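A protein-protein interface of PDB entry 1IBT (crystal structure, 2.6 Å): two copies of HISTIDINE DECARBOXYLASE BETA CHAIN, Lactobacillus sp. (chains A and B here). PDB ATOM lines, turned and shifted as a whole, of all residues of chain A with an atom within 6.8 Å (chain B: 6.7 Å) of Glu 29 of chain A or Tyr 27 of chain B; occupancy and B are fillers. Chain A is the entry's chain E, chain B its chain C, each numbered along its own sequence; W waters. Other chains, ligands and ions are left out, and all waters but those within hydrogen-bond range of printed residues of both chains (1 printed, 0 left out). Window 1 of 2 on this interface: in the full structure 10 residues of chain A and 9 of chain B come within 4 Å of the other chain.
OE2 of Glu 29 of chain A lies within hydrogen-bond range of OH of Tyr 27 of chain B (2.6 Å).
The backbone carbonyl oxygen of Pro 30 of chain A is in hydrogen-bond range of the guanidinium group of Arg 25 of chain A.
The side-chain carboxylate (OE1) of Glu 29 of chain A lies within hydrogen-bond range of the backbone NH (N) of Gly 26 of chain A (2.9 Å).
Pro 30 of chain A touches Tyr 27 of chain B.
CB of Pro 30 of chain A touches O of Gly 34 of chain B, 3.96 Å away.
OD1 of Asn 35 of chain B touches C of Pro 30 of chain A, at 3.6 Å.
CA of Gly 31 of chain A touches ND2 of Asn 35 of chain B (3.5 Å).
Arg 25 of chain A touches none of the printed residues of chain B.
Of the printed residues of chain B, Glu 29 of chain A touches Tyr 27.
Printed residues of chain B within 4 Å of Pro 30 of chain A: Tyr 27, Gly 34 and Asn 35.
Printed residues of chain B within 4 Å of Gly 31 of chain A: Asn 35 (3.5 Å).
Arg 25 of chain B touches none of the printed residues of chain A.
Of the printed residues of chain A, Gly 34 of chain B touches Pro 30 (3.96 Å).
Printed residues of chain A within 4 Å of Asn 35 of chain B: Pro 30 and Gly 31.
The nearest residue of chain B that does not touch Glu 29 of chain A is Met 28 of chain B (4.3 Å).
Of the 12 printed residues of chain B, 3 touch a printed residue of chain A.
Hydrophobic or aromatic side chains of chain B that line the printed part of chain A: Tyr 27.
Among the printed residues, no Asp or Glu carboxylate lies within 4 Å of a Lys or Arg side-chain nitrogen of the other chain.
Glu 29 of chain A touches Tyr 27 of chain B, but with the chains exchanged Tyr 27 of chain A does not touch Glu 29 of chain B (10.3 Å).
6 positions are printed for both chains.
Water W1 lies within hydrogen-bond range of OH of Tyr 20 of chain A (2.7 Å) and O of Asn 35 of chain B (3.1 Å).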
ATOM      1  N   TYR A  20     -27.794  -1.602  18.763  1.00  0.00           N
ATOM      2  CA  TYR A  20     -28.579  -2.292  17.778  1.00  0.00           C
ATOM      3  C   TYR A  20     -28.819  -1.459  16.579  1.00  0.00           C
ATOM      4  O   TYR A  20     -28.549  -0.262  16.537  1.00  0.00           O
ATOM      5  CB  TYR A  20     -29.916  -2.678  18.338  1.00  0.00           C
ATOM      6  CG  TYR A  20     -29.929  -3.701  19.455  1.00  0.00           C
ATOM      7  CD1 TYR A  20     -28.793  -4.455  19.778  1.00  0.00           C
ATOM      8  CD2 TYR A  20     -31.103  -3.854  20.187  1.00  0.00           C
ATOM      9  CE1 TYR A  20     -28.825  -5.354  20.831  1.00  0.00           C
ATOM     10  CE2 TYR A  20     -31.138  -4.757  21.252  1.00  0.00           C
ATOM     11  CZ  TYR A  20     -29.996  -5.496  21.569  1.00  0.00           C
ATOM     12  OH  TYR A  20     -30.020  -6.336  22.664  1.00  0.00           O
ATOM     13  N   THR A  24     -34.162   1.487  19.942  1.00  0.00           N
ATOM     14  CA  THR A  24     -33.583   2.070  21.129  1.00  0.00           C
ATOM     15  C   THR A  24     -33.660   0.897  22.114  1.00  0.00           C
ATOM     16  O   THR A  24     -34.236  -0.176  21.816  1.00  0.00           O
ATOM     17  CB  THR A  24     -34.420   3.225  21.648  1.00  0.00           C
ATOM     18  OG1 THR A  24     -35.783   2.902  21.353  1.00  0.00           O
ATOM     19  CG2 THR A  24     -34.004   4.532  21.058  1.00  0.00           C
ATOM     20  N   ARG A  25     -33.054   1.043  23.289  1.00  0.00           N
ATOM     21  CA  ARG A  25     -33.189   0.046  24.325  1.00  0.00           C
ATOM     22  C   ARG A  25     -33.025   0.738  25.661  1.00  0.00           C
ATOM     23  O   ARG A  25     -32.784   1.953  25.696  1.00  0.00           O
ATOM     24  CB  ARG A  25     -32.176  -1.064  24.036  1.00  0.00           C
ATOM     25  CG  ARG A  25     -30.766  -0.677  23.695  1.00  0.00           C
ATOM     26  CD  ARG A  25     -30.053  -1.805  23.000  1.00  0.00           C
ATOM     27  NE  ARG A  25     -29.915  -3.075  23.678  1.00  0.00           N
ATOM     28  CZ  ARG A  25     -28.987  -3.597  24.503  1.00  0.00           C
ATOM     29  NH1 ARG A  25     -29.222  -4.848  24.876  1.00  0.00           N
ATOM     30  NH2 ARG A  25     -27.931  -2.958  24.990  1.00  0.00           N
ATOM     31  N   GLY A  26     -33.189   0.047  26.759  1.00  0.00           N
ATOM     32  CA  GLY A  26     -33.333   0.692  28.032  1.00  0.00           C
ATOM     33  C   GLY A  26     -32.044   0.987  28.718  1.00  0.00           C
ATOM     34  O   GLY A  26     -31.030   0.350  28.522  1.00  0.00           O
ATOM     35  N   TYR A  27     -32.088   2.012  29.524  1.00  0.00           N
ATOM     36  CA  TYR A  27     -30.986   2.412  30.338  1.00  0.00           C
ATOM     37  C   TYR A  27     -30.744   1.231  31.257  1.00  0.00           C
ATOM     38  O   TYR A  27     -31.698   0.568  31.679  1.00  0.00           O
ATOM     39  CB  TYR A  27     -31.384   3.625  31.104  1.00  0.00           C
ATOM     40  CG  TYR A  27     -30.426   3.996  32.210  1.00  0.00           C
ATOM     41  CD1 TYR A  27     -29.182   4.506  31.901  1.00  0.00           C
ATOM     42  CD2 TYR A  27     -30.802   3.853  33.546  1.00  0.00           C
ATOM     43  CE1 TYR A  27     -28.316   4.875  32.923  1.00  0.00           C
ATOM     44  CE2 TYR A  27     -29.934   4.226  34.571  1.00  0.00           C
ATOM     45  CZ  TYR A  27     -28.697   4.735  34.238  1.00  0.00           C
ATOM     46  OH  TYR A  27     -27.838   5.130  35.204  1.00  0.00           O
ATOM     47  N   MET A  28     -29.449   1.009  31.531  1.00  0.00           N
ATOM     48  CA  MET A  28     -28.896  -0.076  32.314  1.00  0.00           C
ATOM     49  C   MET A  28     -28.831  -1.400  31.571  1.00  0.00           C
ATOM     50  O   MET A  28     -28.258  -2.352  32.087  1.00  0.00           O
ATOM     51  CB  MET A  28     -29.667  -0.319  33.614  1.00  0.00           C
ATOM     52  CG  MET A  28     -29.447   0.797  34.583  1.00  0.00           C
ATOM     53  SD  MET A  28     -30.228   0.670  36.215  1.00  0.00           S
ATOM     54  CE  MET A  28     -31.927   0.819  35.761  1.00  0.00           C
ATOM     55  N   GLU A  29     -29.326  -1.581  30.359  1.00  0.00           N
ATOM     56  CA  GLU A  29     -29.214  -2.872  29.718  1.00  0.00           C
ATOM     57  C   GLU A  29     -27.788  -3.136  29.312  1.00  0.00           C
ATOM     58  O   GLU A  29     -27.088  -2.176  28.966  1.00  0.00           O
ATOM     59  CB  GLU A  29     -30.097  -2.939  28.495  1.00  0.00           C
ATOM     60  CG  GLU A  29     -31.567  -2.773  28.773  1.00  0.00           C
ATOM     61  CD  GLU A  29     -32.442  -3.421  27.749  1.00  0.00           C
ATOM     62  OE1 GLU A  29     -32.873  -2.798  26.809  1.00  0.00           O
ATOM     63  OE2 GLU A  29     -32.726  -4.588  27.842  1.00  0.00           O
ATOM     64  N   PRO A  30     -27.261  -4.373  29.319  1.00  0.00           N
ATOM     65  CA  PRO A  30     -25.886  -4.686  28.993  1.00  0.00           C
ATOM     66  C   PRO A  30     -25.600  -4.418  27.519  1.00  0.00           C
ATOM     67  O   PRO A  30     -26.450  -4.621  26.626  1.00  0.00           O
ATOM     68  CB  PRO A  30     -25.743  -6.125  29.390  1.00  0.00           C
ATOM     69  CG  PRO A  30     -27.062  -6.701  29.010  1.00  0.00           C
ATOM     70  CD  PRO A  30     -27.982  -5.622  29.543  1.00  0.00           C
ATOM     71  N   GLY A  31     -24.412  -3.863  27.255  1.00  0.00           N
ATOM     72  CA  GLY A  31     -23.975  -3.605  25.898  1.00  0.00           C
ATOM     73  C   GLY A  31     -24.288  -2.201  25.443  1.00  0.00           C
ATOM     74  O   GLY A  31     -23.995  -1.826  24.312  1.00  0.00           O
ATOM     75  N   ASN A  32     -24.935  -1.413  26.259  1.00  0.00           N
ATOM     76  CA  ASN A  32     -25.158  -0.063  25.866  1.00  0.00           C
ATOM     77  C   ASN A  32     -23.839   0.614  26.078  1.00  0.00           C
ATOM     78  O   ASN A  32     -23.090   0.232  26.973  1.00  0.00           O
ATOM     79  CB  ASN A  32     -26.234   0.579  26.724  1.00  0.00           C
ATOM     80  CG  ASN A  32     -27.625   0.330  26.204  1.00  0.00           C
ATOM     81  OD1 ASN A  32     -27.885  -0.366  25.230  1.00  0.00           O
ATOM     82  ND2 ASN A  32     -28.595   0.865  26.887  1.00  0.00           N
ATOM     83  N   ILE A  33     -23.516   1.584  25.254  1.00  0.00           N
ATOM     84  CA  ILE A  33     -22.295   2.345  25.383  1.00  0.00           C
ATOM     85  C   ILE A  33     -22.663   3.648  26.065  1.00  0.00           C
ATOM     86  O   ILE A  33     -23.593   4.320  25.657  1.00  0.00           O
ATOM     87  CB  ILE A  33     -21.704   2.560  23.963  1.00  0.00           C
ATOM     88  CG1 ILE A  33     -21.238   1.220  23.444  1.00  0.00           C
ATOM     89  CG2 ILE A  33     -20.577   3.578  23.971  1.00  0.00           C
ATOM     90  CD1 ILE A  33     -20.819   1.173  21.970  1.00  0.00           C
ATOM     91  N   ALA B  16     -25.977 -15.148  27.641  1.00  0.00           N
ATOM     92  CA  ALA B  16     -26.308 -14.773  29.011  1.00  0.00           C
ATOM     93  C   ALA B  16     -25.522 -15.666  29.945  1.00  0.00           C
ATOM     94  O   ALA B  16     -25.955 -16.808  30.169  1.00  0.00           O
ATOM     95  CB  ALA B  16     -27.797 -14.998  29.289  1.00  0.00           C
ATOM     96  N   ARG B  25     -28.072 -15.986  37.860  1.00  0.00           N
ATOM     97  CA  ARG B  25     -28.290 -14.674  38.420  1.00  0.00           C
ATOM     98  C   ARG B  25     -29.064 -13.852  37.398  1.00  0.00           C
ATOM     99  O   ARG B  25     -29.360 -14.342  36.304  1.00  0.00           O
ATOM    100  CB  ARG B  25     -26.923 -14.117  38.822  1.00  0.00           C
ATOM    101  CG  ARG B  25     -25.786 -14.303  37.857  1.00  0.00           C
ATOM    102  CD  ARG B  25     -24.428 -14.047  38.467  1.00  0.00           C
ATOM    103  NE  ARG B  25     -24.201 -12.808  39.167  1.00  0.00           N
ATOM    104  CZ  ARG B  25     -23.635 -11.646  38.832  1.00  0.00           C
ATOM    105  NH1 ARG B  25     -23.582 -10.759  39.810  1.00  0.00           N
ATOM    106  NH2 ARG B  25     -23.245 -11.274  37.628  1.00  0.00           N
ATOM    107  N   GLY B  26     -29.442 -12.638  37.718  1.00  0.00           N
ATOM    108  CA  GLY B  26     -30.416 -11.925  36.936  1.00  0.00           C
ATOM    109  C   GLY B  26     -29.839 -11.165  35.794  1.00  0.00           C
ATOM    110  O   GLY B  26     -28.689 -10.745  35.783  1.00  0.00           O
ATOM    111  N   TYR B  27     -30.668 -11.002  34.791  1.00  0.00           N
ATOM    112  CA  TYR B  27     -30.341 -10.226  33.629  1.00  0.00           C
ATOM    113  C   TYR B  27     -30.136  -8.825  34.154  1.00  0.00           C
ATOM    114  O   TYR B  27     -30.816  -8.403  35.083  1.00  0.00           O
ATOM    115  CB  TYR B  27     -31.494 -10.305  32.683  1.00  0.00           C
ATOM    116  CG  TYR B  27     -31.467  -9.358  31.507  1.00  0.00           C
ATOM    117  CD1 TYR B  27     -30.581  -9.568  30.473  1.00  0.00           C
ATOM    118  CD2 TYR B  27     -32.304  -8.241  31.486  1.00  0.00           C
ATOM    119  CE1 TYR B  27     -30.515  -8.671  29.416  1.00  0.00           C
ATOM    120  CE2 TYR B  27     -32.228  -7.335  30.427  1.00  0.00           C
ATOM    121  CZ  TYR B  27     -31.329  -7.561  29.400  1.00  0.00           C
ATOM    122  OH  TYR B  27     -31.182  -6.667  28.376  1.00  0.00           O
ATOM    123  N   MET B  28     -29.166  -8.157  33.521  1.00  0.00           N
ATOM    124  CA  MET B  28     -28.653  -6.842  33.850  1.00  0.00           C
ATOM    125  C   MET B  28     -27.730  -6.786  35.045  1.00  0.00           C
ATOM    126  O   MET B  28     -27.156  -5.733  35.304  1.00  0.00           O
ATOM    127  CB  MET B  28     -29.778  -5.854  34.093  1.00  0.00           C
ATOM    128  CG  MET B  28     -30.544  -5.564  32.816  1.00  0.00           C
ATOM    129  SD  MET B  28     -31.768  -4.269  32.951  1.00  0.00           S
ATOM    130  CE  MET B  28     -33.006  -5.196  33.793  1.00  0.00           C
ATOM    131  N   GLU B  29     -27.483  -7.846  35.817  1.00  0.00           N
ATOM    132  CA  GLU B  29     -26.582  -7.717  36.953  1.00  0.00           C
ATOM    133  C   GLU B  29     -25.144  -7.549  36.490  1.00  0.00           C
ATOM    134  O   GLU B  29     -24.783  -8.148  35.465  1.00  0.00           O
ATOM    135  CB  GLU B  29     -26.683  -8.938  37.834  1.00  0.00           C
ATOM    136  CG  GLU B  29     -28.028  -9.156  38.431  1.00  0.00           C
ATOM    137  CD  GLU B  29     -27.973  -9.877  39.718  1.00  0.00           C
ATOM    138  OE1 GLU B  29     -28.099 -11.095  39.752  1.00  0.00           O
ATOM    139  OE2 GLU B  29     -27.801  -9.199  40.703  1.00  0.00           O
ATOM    140  N   ASN B  32     -22.128 -10.198  34.411  1.00  0.00           N
ATOM    141  CA  ASN B  32     -22.647 -11.254  33.584  1.00  0.00           C
ATOM    142  C   ASN B  32     -21.977 -11.043  32.260  1.00  0.00           C
ATOM    143  O   ASN B  32     -21.629  -9.914  31.897  1.00  0.00           O
ATOM    144  CB  ASN B  32     -24.144 -11.121  33.454  1.00  0.00           C
ATOM    145  CG  ASN B  32     -24.926 -11.813  34.563  1.00  0.00           C
ATOM    146  OD1 ASN B  32     -24.381 -12.388  35.510  1.00  0.00           O
ATOM    147  ND2 ASN B  32     -26.243 -11.776  34.505  1.00  0.00           N
ATOM    148  N   GLY B  34     -22.325 -11.351  28.296  1.00  0.00           N
ATOM    149  CA  GLY B  34     -23.326 -11.516  27.267  1.00  0.00           C
ATOM    150  C   GLY B  34     -24.350 -10.414  27.351  1.00  0.00           C
ATOM    151  O   GLY B  34     -24.452  -9.733  28.381  1.00  0.00           O
ATOM    152  N   ASN B  35     -25.080 -10.228  26.258  1.00  0.00           N
ATOM    153  CA  ASN B  35     -26.064  -9.181  26.239  1.00  0.00           C
ATOM    154  C   ASN B  35     -27.500  -9.655  26.076  1.00  0.00           C
ATOM    155  O   ASN B  35     -28.377  -8.899  25.680  1.00  0.00           O
ATOM    156  CB  ASN B  35     -25.690  -8.236  25.140  1.00  0.00           C
ATOM    157  CG  ASN B  35     -24.438  -7.434  25.354  1.00  0.00           C
ATOM    158  OD1 ASN B  35     -23.836  -7.367  26.420  1.00  0.00           O
ATOM    159  ND2 ASN B  35     -24.024  -6.706  24.346  1.00  0.00           N
ATOM    160  N   GLY B  36     -27.786 -10.892  26.409  1.00  0.00           N
ATOM    161  CA  GLY B  36     -29.102 -11.461  26.288  1.00  0.00           C
ATOM    162  C   GLY B  36     -29.577 -12.025  27.625  1.00  0.00           C
ATOM    163  O   GLY B  36     -28.938 -11.823  28.657  1.00  0.00           O
ATOM    164  N   TYR B  37     -30.688 -12.764  27.594  1.00  0.00           N
ATOM    165  CA  TYR B  37     -31.286 -13.342  28.771  1.00  0.00           C
ATOM    166  C   TYR B  37     -31.979 -14.662  28.508  1.00  0.00           C
ATOM    167  O   TYR B  37     -32.385 -14.950  27.381  1.00  0.00           O
ATOM    168  CB  TYR B  37     -32.294 -12.373  29.382  1.00  0.00           C
ATOM    169  CG  TYR B  37     -33.417 -11.847  28.494  1.00  0.00           C
ATOM    170  CD1 TYR B  37     -34.458 -12.661  28.048  1.00  0.00           C
ATOM    171  CD2 TYR B  37     -33.416 -10.511  28.131  1.00  0.00           C
ATOM    172  CE1 TYR B  37     -35.477 -12.149  27.252  1.00  0.00           C
ATOM    173  CE2 TYR B  37     -34.435  -9.995  27.345  1.00  0.00           C
ATOM    174  CZ  TYR B  37     -35.453 -10.813  26.914  1.00  0.00           C
ATOM    175  OH  TYR B  37     -36.465 -10.284  26.146  1.00  0.00           O
ATOM    176  N   VAL B  38     -32.122 -15.477  29.555  1.00  0.00           N
ATOM    177  CA  VAL B  38     -32.855 -16.736  29.481  1.00  0.00           C
ATOM    178  C   VAL B  38     -34.014 -16.591  30.458  1.00  0.00           C
ATOM    179  O   VAL B  38     -33.866 -15.956  31.501  1.00  0.00           O
ATOM    180  CB  VAL B  38     -31.989 -17.931  29.887  1.00  0.00           C
ATOM    181  CG1 VAL B  38     -32.709 -19.217  29.658  1.00  0.00           C
ATOM    182  CG2 VAL B  38     -30.818 -18.048  28.974  1.00  0.00           C
HETATM  183  O   HOH W   1     -28.410  -8.521  22.596  1.00  0.00           O
